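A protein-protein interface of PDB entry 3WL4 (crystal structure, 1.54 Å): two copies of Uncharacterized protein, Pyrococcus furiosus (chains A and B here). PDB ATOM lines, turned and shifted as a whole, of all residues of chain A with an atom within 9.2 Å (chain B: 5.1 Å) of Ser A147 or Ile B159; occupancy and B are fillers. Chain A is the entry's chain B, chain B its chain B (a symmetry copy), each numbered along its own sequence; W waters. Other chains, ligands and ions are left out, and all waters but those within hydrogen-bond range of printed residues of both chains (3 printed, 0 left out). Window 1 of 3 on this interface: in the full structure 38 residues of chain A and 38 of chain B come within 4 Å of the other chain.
The side-chain carboxylate (OE1) of Glu A146 lies within hydrogen-bond range of a ring nitrogen (ND1) of His B259, 2.7 Å away. The backbone NH of Ser A147 lies within hydrogen-bond range of the backbone carbonyl oxygen of Tyr B258 (2.8 Å). The guanidinium group of Arg A152 lies within salt-bridge range of the side-chain carboxylate of Glu B160 (3.1 Å). The backbone carbonyl oxygen of Tyr A145 sits close to the backbone carbonyl oxygen of Tyr B258, at 3.0 Å.
The backbone carbonyl oxygen (O) of Tyr A145 sits at hydrogen-bond distance from the side-chain hydroxyl (OG) of Ser A147 (3.0 Å). OE1 of Glu A146 sits at hydrogen-bond distance from N of His A148 (2.8 Å). The guanidinium group (NH1) of Arg A152 sits at hydrogen-bond distance from the backbone carbonyl oxygen (O) of Glu A146 (2.9 Å). NE2 of His A148 is in hydrogen-bond range of OD2 of Asp A150 (3.2 Å).
Tyr A145 touches Trp B142. Glu A146 touches Trp B142 (O to CZ2, 3.7 Å). Glu A146 touches Tyr B258 (C to O, 3.7 Å). Trp B142 touches Ser A147 (CH2 to OG, 3.3 Å). Ile B159 touches Ser A147. Ser A147 touches Glu B160. CB of His A148 touches CE1 of His B259 (3.5 Å). NE2 of His A151 touches CE1 of His B259 (3.4 Å). Arg A152 touches Phe B156.
Leu A143 touches none of the printed residues of chain B. Of the printed residues of chain B, Glu A146 touches Trp B142, Tyr B258 and His B259. Of chain B, only Trp B142, Ile B159, Glu B160 and Tyr B258 come within 4 Å of Ser A147. Printed residues of chain A within 4 Å of Phe B156: Arg A152 (3.7 Å). Of chain A, only Ser A147 comes within 4 Å of Ile B159. Val B162 touches none of the printed residues of chain A. The nearest printed residue of chain B that does not touch Arg A152 is Trp B142 (4.9 Å).
Of the 16 printed residues of chain B, 6 touch a printed residue of chain A. Hydrophobic or aromatic side chains of chain B within 4 Å of the printed part of chain A: Trp B142, Phe B156, Ile B159, Tyr B258 and His B259. Along chain A the printed residues that touch a printed residue of chain B span positions 145 to 152.
Position printed for both chains: 141. Of the 13 pairs that touch across the chains among the printed residues, none has its exchanged pair printed and touching as well.
Water W1 lies within hydrogen-bond range of O of Ser A147 (2.7 Å), OE2 of Glu B160 (2.7 Å) and NH1 of Arg A152 (2.8 Å). Water W2 bridges the backbone carbonyl oxygen of Glu A146 and the indole nitrogen of Trp B142. Water W3 bridges O of Pro A144 (3.2 Å) and N of His B259 (3.3 Å).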
ATOM      1  N   HIS A  40      19.531  16.760  -6.651  1.00  0.00           N
ATOM      2  CA  HIS A  40      19.810  18.072  -7.151  1.00  0.00           C
ATOM      3  C   HIS A  40      18.658  19.053  -6.793  1.00  0.00           C
ATOM      4  O   HIS A  40      17.586  18.576  -6.469  1.00  0.00           O
ATOM      5  CB  HIS A  40      19.789  18.021  -8.742  1.00  0.00           C
ATOM      6  CG  HIS A  40      20.761  16.996  -9.271  1.00  0.00           C
ATOM      7  ND1 HIS A  40      20.339  15.888  -9.964  1.00  0.00           N
ATOM      8  CD2 HIS A  40      22.129  16.929  -9.214  1.00  0.00           C
ATOM      9  CE1 HIS A  40      21.379  15.160 -10.314  1.00  0.00           C
ATOM     10  NE2 HIS A  40      22.489  15.772  -9.889  1.00  0.00           N
ATOM     11  N   THR A 112      27.314  15.805 -10.269  1.00  0.00           N
ATOM     12  CA  THR A 112      28.023  14.730 -11.017  1.00  0.00           C
ATOM     13  C   THR A 112      29.172  14.149 -10.250  1.00  0.00           C
ATOM     14  O   THR A 112      29.834  13.232 -10.758  1.00  0.00           O
ATOM     15  CB  THR A 112      28.519  15.060 -12.454  1.00  0.00           C
ATOM     16  OG1 THR A 112      29.587  16.019 -12.469  1.00  0.00           O
ATOM     17  CG2 THR A 112      27.295  15.668 -13.298  1.00  0.00           C
ATOM     18  N   ASP A 140      14.225   6.051  -5.446  1.00  0.00           N
ATOM     19  CA  ASP A 140      14.426   4.611  -5.446  1.00  0.00           C
ATOM     20  C   ASP A 140      15.687   4.309  -6.252  1.00  0.00           C
ATOM     21  O   ASP A 140      15.760   4.514  -7.479  1.00  0.00           O
ATOM     22  CB  ASP A 140      13.194   4.035  -6.137  1.00  0.00           C
ATOM     23  CG  ASP A 140      13.199   2.568  -6.257  1.00  0.00           C
ATOM     24  OD1 ASP A 140      14.253   1.910  -6.040  1.00  0.00           O
ATOM     25  OD2 ASP A 140      12.111   1.918  -6.556  1.00  0.00           O
ATOM     26  N   PRO A 141      16.744   3.799  -5.584  1.00  0.00           N
ATOM     27  CA  PRO A 141      17.994   3.587  -6.346  1.00  0.00           C
ATOM     28  C   PRO A 141      17.948   2.404  -7.282  1.00  0.00           C
ATOM     29  O   PRO A 141      18.874   2.280  -8.085  1.00  0.00           O
ATOM     30  CB  PRO A 141      19.033   3.328  -5.195  1.00  0.00           C
ATOM     31  CG  PRO A 141      18.192   2.613  -4.075  1.00  0.00           C
ATOM     32  CD  PRO A 141      16.765   3.390  -4.145  1.00  0.00           C
ATOM     33  N   LEU A 143      15.585   2.115  -9.567  1.00  0.00           N
ATOM     34  CA  LEU A 143      14.761   2.504 -10.804  1.00  0.00           C
ATOM     35  C   LEU A 143      15.443   1.937 -12.059  1.00  0.00           C
ATOM     36  O   LEU A 143      16.616   2.227 -12.297  1.00  0.00           O
ATOM     37  CB  LEU A 143      14.742   4.024 -10.842  1.00  0.00           C
ATOM     38  CG  LEU A 143      13.950   4.540 -12.089  1.00  0.00           C
ATOM     39  CD1 LEU A 143      12.397   4.178 -11.929  1.00  0.00           C
ATOM     40  CD2 LEU A 143      14.132   6.076 -12.203  1.00  0.00           C
ATOM     41  N   PRO A 144      14.711   1.178 -12.901  1.00  0.00           N
ATOM     42  CA  PRO A 144      15.438   0.633 -14.067  1.00  0.00           C
ATOM     43  C   PRO A 144      15.953   1.752 -15.001  1.00  0.00           C
ATOM     44  O   PRO A 144      15.243   2.801 -15.207  1.00  0.00           O
ATOM     45  CB  PRO A 144      14.320  -0.212 -14.807  1.00  0.00           C
ATOM     46  CG  PRO A 144      13.438  -0.683 -13.565  1.00  0.00           C
ATOM     47  CD  PRO A 144      13.381   0.578 -12.630  1.00  0.00           C
ATOM     48  N   TYR A 145      17.134   1.549 -15.542  1.00  0.00           N
ATOM     49  CA  TYR A 145      17.803   2.394 -16.524  1.00  0.00           C
ATOM     50  C   TYR A 145      18.134   3.762 -15.947  1.00  0.00           C
ATOM     51  O   TYR A 145      18.520   4.650 -16.728  1.00  0.00           O
ATOM     52  CB  TYR A 145      16.852   2.587 -17.794  1.00  0.00           C
ATOM     53  CG  TYR A 145      16.631   1.214 -18.463  1.00  0.00           C
ATOM     54  CD1 TYR A 145      17.730   0.610 -19.062  1.00  0.00           C
ATOM     55  CD2 TYR A 145      15.392   0.609 -18.421  1.00  0.00           C
ATOM     56  CE1 TYR A 145      17.531  -0.700 -19.635  1.00  0.00           C
ATOM     57  CE2 TYR A 145      15.216  -0.666 -19.026  1.00  0.00           C
ATOM     58  CZ  TYR A 145      16.307  -1.263 -19.593  1.00  0.00           C
ATOM     59  OH  TYR A 145      16.148  -2.563 -20.096  1.00  0.00           O
ATOM     60  N   GLU A 146      18.109   3.923 -14.586  1.00  0.00           N
ATOM     61  CA  GLU A 146      18.564   5.207 -14.086  1.00  0.00           C
ATOM     62  C   GLU A 146      20.045   5.412 -14.306  1.00  0.00           C
ATOM     63  O   GLU A 146      20.824   4.583 -13.730  1.00  0.00           O
ATOM     64  CB  GLU A 146      18.221   5.290 -12.602  1.00  0.00           C
ATOM     65  CG  GLU A 146      18.747   6.596 -11.932  1.00  0.00           C
ATOM     66  CD  GLU A 146      18.321   7.865 -12.742  1.00  0.00           C
ATOM     67  OE1 GLU A 146      19.182   8.556 -13.265  1.00  0.00           O
ATOM     68  OE2 GLU A 146      17.082   8.068 -12.687  1.00  0.00           O
ATOM     69  N   SER A 147      20.474   6.403 -15.083  1.00  0.00           N
ATOM     70  CA  SER A 147      21.867   6.494 -15.478  1.00  0.00           C
ATOM     71  C   SER A 147      22.616   7.635 -14.789  1.00  0.00           C
ATOM     72  O   SER A 147      23.813   7.837 -15.108  1.00  0.00           O
ATOM     73  CB  SER A 147      21.877   6.756 -16.995  1.00  0.00           C
ATOM     74  OG  SER A 147      21.258   5.578 -17.633  1.00  0.00           O
ATOM     75  N   HIS A 148      21.947   8.321 -13.853  1.00  0.00           N
ATOM     76  CA  HIS A 148      22.698   9.422 -13.227  1.00  0.00           C
ATOM     77  C   HIS A 148      23.270   8.863 -11.849  1.00  0.00           C
ATOM     78  O   HIS A 148      22.482   8.542 -10.927  1.00  0.00           O
ATOM     79  CB  HIS A 148      21.713  10.603 -12.921  1.00  0.00           C
ATOM     80  CG  HIS A 148      22.513  11.840 -12.706  1.00  0.00           C
ATOM     81  ND1 HIS A 148      22.346  13.065 -13.338  1.00  0.00           N
ATOM     82  CD2 HIS A 148      23.613  11.978 -11.900  1.00  0.00           C
ATOM     83  CE1 HIS A 148      23.330  13.903 -12.960  1.00  0.00           C
ATOM     84  NE2 HIS A 148      24.098  13.236 -12.052  1.00  0.00           N
ATOM     85  N   PRO A 149      24.590   8.832 -11.748  1.00  0.00           N
ATOM     86  CA  PRO A 149      25.121   8.281 -10.446  1.00  0.00           C
ATOM     87  C   PRO A 149      24.661   9.107  -9.239  1.00  0.00           C
ATOM     88  O   PRO A 149      24.573   8.523  -8.151  1.00  0.00           O
ATOM     89  CB  PRO A 149      26.666   8.366 -10.649  1.00  0.00           C
ATOM     90  CG  PRO A 149      26.885   9.483 -11.756  1.00  0.00           C
ATOM     91  CD  PRO A 149      25.639   9.303 -12.720  1.00  0.00           C
ATOM     92  N   ASP A 150      24.470  10.454  -9.428  1.00  0.00           N
ATOM     93  CA  ASP A 150      24.039  11.191  -8.211  1.00  0.00           C
ATOM     94  C   ASP A 150      22.695  10.667  -7.724  1.00  0.00           C
ATOM     95  O   ASP A 150      22.360  10.719  -6.540  1.00  0.00           O
ATOM     96  CB  ASP A 150      23.860  12.696  -8.473  1.00  0.00           C
ATOM     97  CG  ASP A 150      25.113  13.406  -8.818  1.00  0.00           C
ATOM     98  OD1 ASP A 150      26.289  12.958  -8.577  1.00  0.00           O
ATOM     99  OD2 ASP A 150      25.020  14.592  -9.312  1.00  0.00           O
ATOM    100  N   HIS A 151      21.798  10.267  -8.675  1.00  0.00           N
ATOM    101  CA  HIS A 151      20.471   9.737  -8.229  1.00  0.00           C
ATOM    102  C   HIS A 151      20.624   8.383  -7.548  1.00  0.00           C
ATOM    103  O   HIS A 151      20.026   8.137  -6.477  1.00  0.00           O
ATOM    104  CB  HIS A 151      19.538   9.635  -9.465  1.00  0.00           C
ATOM    105  CG  HIS A 151      18.875  10.948  -9.746  1.00  0.00           C
ATOM    106  ND1 HIS A 151      17.511  11.041  -9.919  1.00  0.00           N
ATOM    107  CD2 HIS A 151      19.414  12.189  -9.862  1.00  0.00           C
ATOM    108  CE1 HIS A 151      17.214  12.328 -10.143  1.00  0.00           C
ATOM    109  NE2 HIS A 151      18.318  13.065 -10.119  1.00  0.00           N
ATOM    110  N   ARG A 152      21.361   7.444  -8.157  1.00  0.00           N
ATOM    111  CA  ARG A 152      21.492   6.088  -7.558  1.00  0.00           C
ATOM    112  C   ARG A 152      22.133   6.254  -6.157  1.00  0.00           C
ATOM    113  O   ARG A 152      21.632   5.676  -5.167  1.00  0.00           O
ATOM    114  CB  ARG A 152      22.414   5.212  -8.436  1.00  0.00           C
ATOM    115  CG  ARG A 152      21.817   4.927  -9.807  1.00  0.00           C
ATOM    116  CD  ARG A 152      22.701   3.892 -10.529  1.00  0.00           C
ATOM    117  NE  ARG A 152      24.028   4.420 -10.854  1.00  0.00           N
ATOM    118  CZ  ARG A 152      24.445   4.734 -12.044  1.00  0.00           C
ATOM    119  NH1 ARG A 152      23.680   4.749 -13.165  1.00  0.00           N
ATOM    120  NH2 ARG A 152      25.707   5.124 -12.229  1.00  0.00           N
ATOM    121  N   ARG A 153      23.211   7.046  -6.173  1.00  0.00           N
ATOM    122  CA  ARG A 153      23.955   7.190  -4.837  1.00  0.00           C
ATOM    123  C   ARG A 153      23.045   7.822  -3.764  1.00  0.00           C
ATOM    124  O   ARG A 153      23.097   7.440  -2.620  1.00  0.00           O
ATOM    125  CB  ARG A 153      25.230   7.948  -5.015  1.00  0.00           C
ATOM    126  CG  ARG A 153      26.244   7.026  -5.830  1.00  0.00           C
ATOM    127  CD  ARG A 153      27.417   7.860  -6.235  1.00  0.00           C
ATOM    128  NE  ARG A 153      28.376   6.945  -6.882  1.00  0.00           N
ATOM    129  CZ  ARG A 153      29.683   7.189  -6.963  1.00  0.00           C
ATOM    130  NH1 ARG A 153      30.218   8.354  -6.590  1.00  0.00           N
ATOM    131  NH2 ARG A 153      30.468   6.169  -7.463  1.00  0.00           N
ATOM    132  N   PRO B 141      24.989  -1.981 -19.182  1.00  0.00           N
ATOM    133  CA  PRO B 141      25.491  -2.289 -17.824  1.00  0.00           C
ATOM    134  C   PRO B 141      24.471  -2.947 -16.928  1.00  0.00           C
ATOM    135  O   PRO B 141      24.870  -3.404 -15.856  1.00  0.00           O
ATOM    136  CB  PRO B 141      25.848  -0.858 -17.281  1.00  0.00           C
ATOM    137  CG  PRO B 141      24.794   0.085 -17.969  1.00  0.00           C
ATOM    138  CD  PRO B 141      24.664  -0.548 -19.461  1.00  0.00           C
ATOM    139  N   TRP B 142      23.274  -3.045 -17.404  1.00  0.00           N
ATOM    140  CA  TRP B 142      22.202  -3.754 -16.627  1.00  0.00           C
ATOM    141  C   TRP B 142      21.968  -5.180 -17.082  1.00  0.00           C
ATOM    142  O   TRP B 142      21.021  -5.839 -16.580  1.00  0.00           O
ATOM    143  CB  TRP B 142      20.864  -3.023 -16.729  1.00  0.00           C
ATOM    144  CG  TRP B 142      20.955  -1.585 -16.189  1.00  0.00           C
ATOM    145  CD1 TRP B 142      21.014  -1.224 -14.865  1.00  0.00           C
ATOM    146  CD2 TRP B 142      21.122  -0.378 -16.988  1.00  0.00           C
ATOM    147  NE1 TRP B 142      21.123   0.195 -14.769  1.00  0.00           N
ATOM    148  CE2 TRP B 142      21.186   0.696 -16.045  1.00  0.00           C
ATOM    149  CE3 TRP B 142      21.155  -0.106 -18.369  1.00  0.00           C
ATOM    150  CZ2 TRP B 142      21.307   2.058 -16.446  1.00  0.00           C
ATOM    151  CZ3 TRP B 142      21.296   1.247 -18.793  1.00  0.00           C
ATOM    152  CH2 TRP B 142      21.380   2.287 -17.836  1.00  0.00           C
ATOM    153  N   THR B 154      32.225  -0.001 -17.963  1.00  0.00           N
ATOM    154  CA  THR B 154      32.260   0.590 -19.273  1.00  0.00           C
ATOM    155  C   THR B 154      30.904   1.017 -19.675  1.00  0.00           C
ATOM    156  O   THR B 154      30.745   2.116 -20.285  1.00  0.00           O
ATOM    157  CB  THR B 154      32.786  -0.530 -20.244  1.00  0.00           C
ATOM    158  OG1 THR B 154      34.159  -0.811 -19.963  1.00  0.00           O
ATOM    159  CG2 THR B 154      32.783   0.041 -21.718  1.00  0.00           C
ATOM    160  N   GLY B 155      29.835   0.218 -19.474  1.00  0.00           N
ATOM    161  CA  GLY B 155      28.514   0.632 -19.905  1.00  0.00           C
ATOM    162  C   GLY B 155      28.035   1.919 -19.212  1.00  0.00           C
ATOM    163  O   GLY B 155      27.539   2.827 -19.828  1.00  0.00           O
ATOM    164  N   PHE B 156      28.172   1.920 -17.879  1.00  0.00           N
ATOM    165  CA  PHE B 156      27.707   3.130 -17.144  1.00  0.00           C
ATOM    166  C   PHE B 156      28.536   4.326 -17.554  1.00  0.00           C
ATOM    167  O   PHE B 156      27.982   5.411 -17.786  1.00  0.00           O
ATOM    168  CB  PHE B 156      27.860   2.897 -15.609  1.00  0.00           C
ATOM    169  CG  PHE B 156      26.847   1.960 -15.007  1.00  0.00           C
ATOM    170  CD1 PHE B 156      25.492   2.224 -15.173  1.00  0.00           C
ATOM    171  CD2 PHE B 156      27.305   0.840 -14.266  1.00  0.00           C
ATOM    172  CE1 PHE B 156      24.501   1.365 -14.563  1.00  0.00           C
ATOM    173  CE2 PHE B 156      26.315  -0.004 -13.675  1.00  0.00           C
ATOM    174  CZ  PHE B 156      24.942   0.293 -13.842  1.00  0.00           C
ATOM    175  N   LEU B 157      29.846   4.207 -17.604  1.00  0.00           N
ATOM    176  CA  LEU B 157      30.726   5.386 -17.923  1.00  0.00           C
ATOM    177  C   LEU B 157      30.417   5.860 -19.339  1.00  0.00           C
ATOM    178  O   LEU B 157      30.460   7.075 -19.602  1.00  0.00           O
ATOM    179  CB  LEU B 157      32.177   5.042 -17.837  1.00  0.00           C
ATOM    180  CG  LEU B 157      32.663   4.748 -16.392  1.00  0.00           C
ATOM    181  CD1 LEU B 157      34.021   4.015 -16.425  1.00  0.00           C
ATOM    182  CD2 LEU B 157      32.791   6.072 -15.581  1.00  0.00           C
ATOM    183  N   ALA B 158      30.097   4.938 -20.277  1.00  0.00           N
ATOM    184  CA  ALA B 158      29.828   5.413 -21.636  1.00  0.00           C
ATOM    185  C   ALA B 158      28.533   6.192 -21.683  1.00  0.00           C
ATOM    186  O   ALA B 158      28.485   7.283 -22.261  1.00  0.00           O
ATOM    187  CB  ALA B 158      29.585   4.145 -22.533  1.00  0.00           C
ATOM    188  N   ILE B 159      27.466   5.767 -21.020  1.00  0.00           N
ATOM    189  CA  ILE B 159      26.200   6.441 -20.992  1.00  0.00           C
ATOM    190  C   ILE B 159      26.368   7.803 -20.338  1.00  0.00           C
ATOM    191  O   ILE B 159      25.918   8.847 -20.872  1.00  0.00           O
ATOM    192  CB  ILE B 159      25.191   5.607 -20.203  1.00  0.00           C
ATOM    193  CG1 ILE B 159      24.879   4.386 -21.065  1.00  0.00           C
ATOM    194  CG2 ILE B 159      23.882   6.487 -20.061  1.00  0.00           C
ATOM    195  CD1 ILE B 159      24.041   3.299 -20.198  1.00  0.00           C
ATOM    196  N   GLU B 160      27.049   7.827 -19.191  1.00  0.00           N
ATOM    197  CA  GLU B 160      27.259   9.127 -18.485  1.00  0.00           C
ATOM    198  C   GLU B 160      28.100  10.046 -19.347  1.00  0.00           C
ATOM    199  O   GLU B 160      27.805  11.278 -19.375  1.00  0.00           O
ATOM    200  CB  GLU B 160      28.049   8.808 -17.198  1.00  0.00           C
ATOM    201  CG  GLU B 160      27.194   7.959 -16.229  1.00  0.00           C
ATOM    202  CD  GLU B 160      28.063   7.116 -15.232  1.00  0.00           C
ATOM    203  OE1 GLU B 160      29.227   7.344 -15.107  1.00  0.00           O
ATOM    204  OE2 GLU B 160      27.405   6.245 -14.600  1.00  0.00           O
ATOM    205  N   SER B 161      29.132   9.556 -20.021  1.00  0.00           N
ATOM    206  CA  SER B 161      30.046  10.425 -20.757  1.00  0.00           C
ATOM    207  C   SER B 161      29.270  10.974 -21.965  1.00  0.00           C
ATOM    208  O   SER B 161      29.619  12.103 -22.339  1.00  0.00           O
ATOM    209  CB  SER B 161      31.243   9.672 -21.195  1.00  0.00           C
ATOM    210  OG  SER B 161      32.020   9.275 -20.013  1.00  0.00           O
ATOM    211  N   VAL B 162      28.436  10.189 -22.619  1.00  0.00           N
ATOM    212  CA  VAL B 162      27.672  10.795 -23.749  1.00  0.00           C
ATOM    213  C   VAL B 162      26.821  11.960 -23.169  1.00  0.00           C
ATOM    214  O   VAL B 162      26.793  13.061 -23.821  1.00  0.00           O
ATOM    215  CB  VAL B 162      26.779   9.696 -24.344  1.00  0.00           C
ATOM    216  CG1 VAL B 162      25.747  10.353 -25.284  1.00  0.00           C
ATOM    217  CG2 VAL B 162      27.747   8.717 -25.131  1.00  0.00           C
ATOM    218  N   ALA B 163      26.186  11.794 -22.023  1.00  0.00           N
ATOM    219  CA  ALA B 163      25.371  12.919 -21.520  1.00  0.00           C
ATOM    220  C   ALA B 163      26.295  14.069 -21.191  1.00  0.00           C
ATOM    221  O   ALA B 163      25.985  15.255 -21.487  1.00  0.00           O
ATOM    222  CB  ALA B 163      24.634  12.467 -20.256  1.00  0.00           C
ATOM    223  N   ILE B 187      22.575   6.449 -28.670  1.00  0.00           N
ATOM    224  CA  ILE B 187      23.388   5.428 -27.990  1.00  0.00           C
ATOM    225  C   ILE B 187      22.713   4.081 -28.355  1.00  0.00           C
ATOM    226  O   ILE B 187      21.479   3.947 -28.437  1.00  0.00           O
ATOM    227  CB  ILE B 187      23.252   5.585 -26.483  1.00  0.00           C
ATOM    228  CG1 ILE B 187      24.057   6.772 -26.103  1.00  0.00           C
ATOM    229  CG2 ILE B 187      23.841   4.297 -25.724  1.00  0.00           C
ATOM    230  CD1 ILE B 187      23.704   7.082 -24.585  1.00  0.00           C
ATOM    231  N   LEU B 189      23.051  -0.014 -26.962  1.00  0.00           N
ATOM    232  CA  LEU B 189      23.760  -0.907 -25.945  1.00  0.00           C
ATOM    233  C   LEU B 189      23.755  -2.287 -26.563  1.00  0.00           C
ATOM    234  O   LEU B 189      22.672  -2.854 -26.912  1.00  0.00           O
ATOM    235  CB  LEU B 189      22.987  -0.913 -24.637  1.00  0.00           C
ATOM    236  CG  LEU B 189      22.870   0.559 -24.095  1.00  0.00           C
ATOM    237  CD1 LEU B 189      22.034   0.416 -22.813  1.00  0.00           C
ATOM    238  CD2 LEU B 189      24.220   1.132 -23.767  1.00  0.00           C
ATOM    239  N   TYR B 258      16.809   7.390 -19.960  1.00  0.00           N
ATOM    240  CA  TYR B 258      17.957   6.987 -19.075  1.00  0.00           C
ATOM    241  C   TYR B 258      17.893   7.706 -17.779  1.00  0.00           C
ATOM    242  O   TYR B 258      18.897   7.645 -17.053  1.00  0.00           O
ATOM    243  CB  TYR B 258      19.261   7.345 -19.849  1.00  0.00           C
ATOM    244  CG  TYR B 258      19.565   6.434 -21.042  1.00  0.00           C
ATOM    245  CD1 TYR B 258      20.412   5.408 -20.894  1.00  0.00           C
ATOM    246  CD2 TYR B 258      19.078   6.785 -22.313  1.00  0.00           C
ATOM    247  CE1 TYR B 258      20.707   4.545 -21.987  1.00  0.00           C
ATOM    248  CE2 TYR B 258      19.395   5.965 -23.435  1.00  0.00           C
ATOM    249  CZ  TYR B 258      20.156   4.893 -23.237  1.00  0.00           C
ATOM    250  OH  TYR B 258      20.590   4.109 -24.305  1.00  0.00           O
ATOM    251  N   HIS B 259      16.782   8.385 -17.474  1.00  0.00           N
ATOM    252  CA  HIS B 259      16.774   9.150 -16.198  1.00  0.00           C
ATOM    253  C   HIS B 259      15.380   9.347 -15.708  1.00  0.00           C
ATOM    254  O   HIS B 259      14.471   9.762 -16.516  1.00  0.00           O
ATOM    255  CB  HIS B 259      17.453  10.488 -16.472  1.00  0.00           C
ATOM    256  CG  HIS B 259      17.628  11.378 -15.294  1.00  0.00           C
ATOM    257  ND1 HIS B 259      18.289  10.919 -14.128  1.00  0.00           N
ATOM    258  CD2 HIS B 259      17.402  12.699 -15.109  1.00  0.00           C
ATOM    259  CE1 HIS B 259      18.461  11.973 -13.296  1.00  0.00           C
ATOM    260  NE2 HIS B 259      17.924  13.061 -13.854  1.00  0.00           N
HETATM  261  O   HOH W   1      24.989   5.416 -15.580  1.00  0.00           O
HETATM  262  O   HOH W   2      20.748   2.011 -12.646  1.00  0.00           O
HETATM  263  O   HOH W   3      15.052   5.927 -15.998  1.00  0.00           O
